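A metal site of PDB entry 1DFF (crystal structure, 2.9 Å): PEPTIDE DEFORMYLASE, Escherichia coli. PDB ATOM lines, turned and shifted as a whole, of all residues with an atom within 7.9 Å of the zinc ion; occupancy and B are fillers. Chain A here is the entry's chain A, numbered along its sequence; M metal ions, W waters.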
ATOM      1  N   LEU A  13      -2.637 -18.894  13.903  1.00  0.00           N
ATOM      2  CA  LEU A  13      -1.250 -18.587  13.581  1.00  0.00           C
ATOM      3  C   LEU A  13      -0.933 -17.147  13.918  1.00  0.00           C
ATOM      4  O   LEU A  13       0.243 -16.774  14.005  1.00  0.00           O
ATOM      5  CB  LEU A  13      -1.010 -18.776  12.085  1.00  0.00           C
ATOM      6  CG  LEU A  13      -0.731 -20.205  11.647  1.00  0.00           C
ATOM      7  CD1 LEU A  13      -0.922 -20.291  10.150  1.00  0.00           C
ATOM      8  CD2 LEU A  13       0.686 -20.622  12.032  1.00  0.00           C
ATOM      9  N   GLY A  45      13.633 -24.828  12.904  1.00  0.00           N
ATOM     10  CA  GLY A  45      13.187 -24.120  14.093  1.00  0.00           C
ATOM     11  C   GLY A  45      11.676 -24.187  14.069  1.00  0.00           C
ATOM     12  O   GLY A  45      11.083 -24.257  12.982  1.00  0.00           O
ATOM     13  N   LEU A  46      11.029 -24.161  15.232  1.00  0.00           N
ATOM     14  CA  LEU A  46       9.570 -24.247  15.304  1.00  0.00           C
ATOM     15  C   LEU A  46       9.104 -23.516  16.528  1.00  0.00           C
ATOM     16  O   LEU A  46       9.750 -23.614  17.573  1.00  0.00           O
ATOM     17  CB  LEU A  46       9.124 -25.705  15.419  1.00  0.00           C
ATOM     18  CG  LEU A  46       7.634 -25.992  15.618  1.00  0.00           C
ATOM     19  CD1 LEU A  46       6.888 -25.970  14.293  1.00  0.00           C
ATOM     20  CD2 LEU A  46       7.497 -27.362  16.239  1.00  0.00           C
ATOM     21  N   ALA A  47       8.014 -22.798  16.412  1.00  0.00           N
ATOM     22  CA  ALA A  47       7.493 -22.080  17.561  1.00  0.00           C
ATOM     23  C   ALA A  47       6.217 -22.783  18.049  1.00  0.00           C
ATOM     24  O   ALA A  47       5.473 -23.350  17.249  1.00  0.00           O
ATOM     25  CB  ALA A  47       7.205 -20.648  17.168  1.00  0.00           C
ATOM     26  N   GLN A  50       2.839 -22.533  16.153  1.00  0.00           N
ATOM     27  CA  GLN A  50       2.535 -23.270  14.938  1.00  0.00           C
ATOM     28  C   GLN A  50       1.921 -24.623  15.214  1.00  0.00           C
ATOM     29  O   GLN A  50       1.505 -25.314  14.269  1.00  0.00           O
ATOM     30  CB  GLN A  50       3.774 -23.447  14.088  1.00  0.00           C
ATOM     31  CG  GLN A  50       4.389 -22.162  13.721  1.00  0.00           C
ATOM     32  CD  GLN A  50       5.677 -22.396  13.043  1.00  0.00           C
ATOM     33  OE1 GLN A  50       6.731 -22.264  13.640  1.00  0.00           O
ATOM     34  NE2 GLN A  50       5.612 -22.813  11.801  1.00  0.00           N
ATOM     35  N   GLU A  88      14.049 -17.396   2.901  1.00  0.00           N
ATOM     36  CA  GLU A  88      13.614 -18.337   3.902  1.00  0.00           C
ATOM     37  C   GLU A  88      12.221 -18.870   3.754  1.00  0.00           C
ATOM     38  O   GLU A  88      11.353 -18.232   3.154  1.00  0.00           O
ATOM     39  CB  GLU A  88      13.733 -17.701   5.267  1.00  0.00           C
ATOM     40  CG  GLU A  88      13.080 -16.363   5.369  1.00  0.00           C
ATOM     41  CD  GLU A  88      13.329 -15.747   6.712  1.00  0.00           C
ATOM     42  OE1 GLU A  88      14.429 -15.941   7.249  1.00  0.00           O
ATOM     43  OE2 GLU A  88      12.429 -15.074   7.262  1.00  0.00           O
ATOM     44  N   GLY A  89      12.002 -20.011   4.402  1.00  0.00           N
ATOM     45  CA  GLY A  89      10.710 -20.672   4.362  1.00  0.00           C
ATOM     46  C   GLY A  89      10.103 -20.834   5.747  1.00  0.00           C
ATOM     47  O   GLY A  89      10.728 -20.450   6.742  1.00  0.00           O
ATOM     48  N   CYS A  90       8.907 -21.408   5.815  1.00  0.00           N
ATOM     49  CA  CYS A  90       8.205 -21.638   7.070  1.00  0.00           C
ATOM     50  C   CYS A  90       7.302 -22.877   6.877  1.00  0.00           C
ATOM     51  O   CYS A  90       6.635 -23.026   5.851  1.00  0.00           O
ATOM     52  CB  CYS A  90       7.380 -20.404   7.419  1.00  0.00           C
ATOM     53  SG  CYS A  90       6.342 -20.519   8.893  1.00  0.00           S
ATOM     54  N   LEU A  91       7.281 -23.744   7.895  1.00  0.00           N
ATOM     55  CA  LEU A  91       6.506 -25.001   7.872  1.00  0.00           C
ATOM     56  C   LEU A  91       5.003 -24.804   7.834  1.00  0.00           C
ATOM     57  O   LEU A  91       4.269 -25.745   7.532  1.00  0.00           O
ATOM     58  CB  LEU A  91       6.911 -25.871   9.072  1.00  0.00           C
ATOM     59  CG  LEU A  91       8.399 -26.221   9.077  1.00  0.00           C
ATOM     60  CD1 LEU A  91       8.850 -26.571  10.468  1.00  0.00           C
ATOM     61  CD2 LEU A  91       8.692 -27.342   8.106  1.00  0.00           C
ATOM     62  N   SER A  92       4.573 -23.590   8.178  1.00  0.00           N
ATOM     63  CA  SER A  92       3.173 -23.186   8.164  1.00  0.00           C
ATOM     64  C   SER A  92       2.858 -22.564   6.804  1.00  0.00           C
ATOM     65  O   SER A  92       1.703 -22.412   6.441  1.00  0.00           O
ATOM     66  CB  SER A  92       2.922 -22.191   9.280  1.00  0.00           C
ATOM     67  OG  SER A  92       3.305 -22.774  10.518  1.00  0.00           O
ATOM     68  N   ILE A  93       3.909 -22.288   6.031  1.00  0.00           N
ATOM     69  CA  ILE A  93       3.788 -21.724   4.694  1.00  0.00           C
ATOM     70  C   ILE A  93       4.429 -22.684   3.708  1.00  0.00           C
ATOM     71  O   ILE A  93       5.546 -22.472   3.229  1.00  0.00           O
ATOM     72  CB  ILE A  93       4.463 -20.334   4.576  1.00  0.00           C
ATOM     73  CG1 ILE A  93       3.959 -19.424   5.680  1.00  0.00           C
ATOM     74  CG2 ILE A  93       4.148 -19.704   3.205  1.00  0.00           C
ATOM     75  CD1 ILE A  93       4.414 -18.006   5.524  1.00  0.00           C
ATOM     76  N   CYS A 129      17.306 -17.208  11.923  1.00  0.00           N
ATOM     77  CA  CYS A 129      16.345 -18.205  12.394  1.00  0.00           C
ATOM     78  C   CYS A 129      15.644 -17.790  13.704  1.00  0.00           C
ATOM     79  O   CYS A 129      14.419 -17.823  13.787  1.00  0.00           O
ATOM     80  CB  CYS A 129      17.050 -19.551  12.568  1.00  0.00           C
ATOM     81  SG  CYS A 129      15.981 -20.899  12.908  1.00  0.00           S
ATOM     82  N   HIS A 132      13.186 -15.120  12.910  1.00  0.00           N
ATOM     83  CA  HIS A 132      12.044 -15.665  12.215  1.00  0.00           C
ATOM     84  C   HIS A 132      11.086 -16.328  13.179  1.00  0.00           C
ATOM     85  O   HIS A 132       9.899 -16.043  13.129  1.00  0.00           O
ATOM     86  CB  HIS A 132      12.496 -16.640  11.138  1.00  0.00           C
ATOM     87  CG  HIS A 132      11.392 -17.446  10.516  1.00  0.00           C
ATOM     88  ND1 HIS A 132      11.288 -17.701   9.177  1.00  0.00           N
ATOM     89  CD2 HIS A 132      10.397 -18.157  11.097  1.00  0.00           C
ATOM     90  CE1 HIS A 132      10.272 -18.560   8.986  1.00  0.00           C
ATOM     91  NE2 HIS A 132       9.696 -18.857  10.136  1.00  0.00           N
ATOM     92  N   GLU A 133      11.571 -17.166  14.071  1.00  0.00           N
ATOM     93  CA  GLU A 133      10.690 -17.875  15.019  1.00  0.00           C
ATOM     94  C   GLU A 133      10.032 -16.942  16.020  1.00  0.00           C
ATOM     95  O   GLU A 133       8.818 -16.983  16.188  1.00  0.00           O
ATOM     96  CB  GLU A 133      11.416 -19.011  15.797  1.00  0.00           C
ATOM     97  CG  GLU A 133      12.178 -20.067  14.964  1.00  0.00           C
ATOM     98  CD  GLU A 133      11.296 -20.844  14.018  1.00  0.00           C
ATOM     99  OE1 GLU A 133      10.137 -21.135  14.405  1.00  0.00           O
ATOM    100  OE2 GLU A 133      11.769 -21.151  12.906  1.00  0.00           O
ATOM    101  N   ASP A 135       9.030 -14.116  15.800  1.00  0.00           N
ATOM    102  CA  ASP A 135       7.904 -13.423  15.154  1.00  0.00           C
ATOM    103  C   ASP A 135       6.664 -14.262  15.399  1.00  0.00           C
ATOM    104  O   ASP A 135       5.605 -13.760  15.771  1.00  0.00           O
ATOM    105  CB  ASP A 135       8.092 -13.289  13.635  1.00  0.00           C
ATOM    106  CG  ASP A 135       8.851 -12.024  13.220  1.00  0.00           C
ATOM    107  OD1 ASP A 135       9.083 -11.120  14.059  1.00  0.00           O
ATOM    108  OD2 ASP A 135       9.221 -11.949  12.013  1.00  0.00           O
ATOM    109  N   HIS A 136       6.798 -15.556  15.191  1.00  0.00           N
ATOM    110  CA  HIS A 136       5.683 -16.448  15.388  1.00  0.00           C
ATOM    111  C   HIS A 136       5.017 -16.214  16.725  1.00  0.00           C
ATOM    112  O   HIS A 136       3.813 -16.010  16.755  1.00  0.00           O
ATOM    113  CB  HIS A 136       6.148 -17.890  15.297  1.00  0.00           C
ATOM    114  CG  HIS A 136       6.176 -18.411  13.911  1.00  0.00           C
ATOM    115  ND1 HIS A 136       5.140 -18.263  13.022  1.00  0.00           N
ATOM    116  CD2 HIS A 136       7.133 -19.105  13.255  1.00  0.00           C
ATOM    117  CE1 HIS A 136       5.483 -18.865  11.870  1.00  0.00           C
ATOM    118  NE2 HIS A 136       6.693 -19.403  11.962  1.00  0.00           N
ATOM    119  N   LYS A 140       3.382 -13.011  13.998  1.00  0.00           N
ATOM    120  CA  LYS A 140       3.917 -12.331  12.809  1.00  0.00           C
ATOM    121  C   LYS A 140       4.546 -13.297  11.827  1.00  0.00           C
ATOM    122  O   LYS A 140       5.460 -14.021  12.178  1.00  0.00           O
ATOM    123  CB  LYS A 140       4.930 -11.290  13.273  1.00  0.00           C
ATOM    124  CG  LYS A 140       5.218 -10.140  12.344  1.00  0.00           C
ATOM    125  CD  LYS A 140       6.044  -9.140  13.104  1.00  0.00           C
ATOM    126  CE  LYS A 140       6.804  -8.203  12.208  1.00  0.00           C
ATOM    127  NZ  LYS A 140       7.504  -7.186  13.061  1.00  0.00           N
ATOM    128  N   LEU A 141       4.090 -13.281  10.576  1.00  0.00           N
ATOM    129  CA  LEU A 141       4.617 -14.163   9.540  1.00  0.00           C
ATOM    130  C   LEU A 141       5.594 -13.508   8.552  1.00  0.00           C
ATOM    131  O   LEU A 141       5.439 -12.351   8.215  1.00  0.00           O
ATOM    132  CB  LEU A 141       3.448 -14.835   8.806  1.00  0.00           C
ATOM    133  CG  LEU A 141       2.833 -15.966   9.641  1.00  0.00           C
ATOM    134  CD1 LEU A 141       1.324 -16.012   9.517  1.00  0.00           C
ATOM    135  CD2 LEU A 141       3.472 -17.274   9.191  1.00  0.00           C
ATOM    136  N   PHE A 142       6.588 -14.256   8.062  1.00  0.00           N
ATOM    137  CA  PHE A 142       7.574 -13.667   7.157  1.00  0.00           C
ATOM    138  C   PHE A 142       6.936 -13.028   5.965  1.00  0.00           C
ATOM    139  O   PHE A 142       7.400 -11.999   5.480  1.00  0.00           O
ATOM    140  CB  PHE A 142       8.673 -14.683   6.718  1.00  0.00           C
ATOM    141  CG  PHE A 142       8.257 -15.693   5.644  1.00  0.00           C
ATOM    142  CD1 PHE A 142       8.393 -15.393   4.293  1.00  0.00           C
ATOM    143  CD2 PHE A 142       7.811 -16.956   5.988  1.00  0.00           C
ATOM    144  CE1 PHE A 142       8.087 -16.347   3.312  1.00  0.00           C
ATOM    145  CE2 PHE A 142       7.514 -17.919   5.000  1.00  0.00           C
ATOM    146  CZ  PHE A 142       7.660 -17.610   3.666  1.00  0.00           C
HETATM  147 ZN    ZN M   1       7.909 -20.090  10.458  1.00  0.00          ZN
HETATM  148  O   HOH W   1       8.878 -22.206  10.694  1.00  0.00           O
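OE1 of Gln 50 sits at hydrogen-bond distance from N of Ala 47 (3.1 Å). The side-chain sulfur (SG) of Cys 90 lies close to the backbone NH (N) of Ser 92, at 3.6 Å. The side-chain hydroxyl of Ser 92 lies within hydrogen-bond range of the side-chain amide nitrogen of Gln 50, 2.6 Å away. OE1 of Gln 50 sits close to NE2 of His 136 (3.3 Å). The side-chain sulfur of Cys 90 sits close to the side-chain amide nitrogen of Gln 50 (3.8 Å). ND1 of His 132 is in hydrogen-bond range of OE2 of Glu 88 (3.4 Å).
The zinc ion is bound by a ring nitrogen (NE2) of His 136 (2.1 Å), a ring nitrogen (NE2) of His 132 (2.2 Å), the side-chain sulfur of Cys 90 (2.3 Å) and water W1 (2.3 Å). The zinc ion has four donor atoms within binding distance.
Merely in contact with the zinc ion: Gln 50. Four residues have an atom within 4 Å of the zinc ion: Gln 50, Cys 90, His 132 and His 136.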
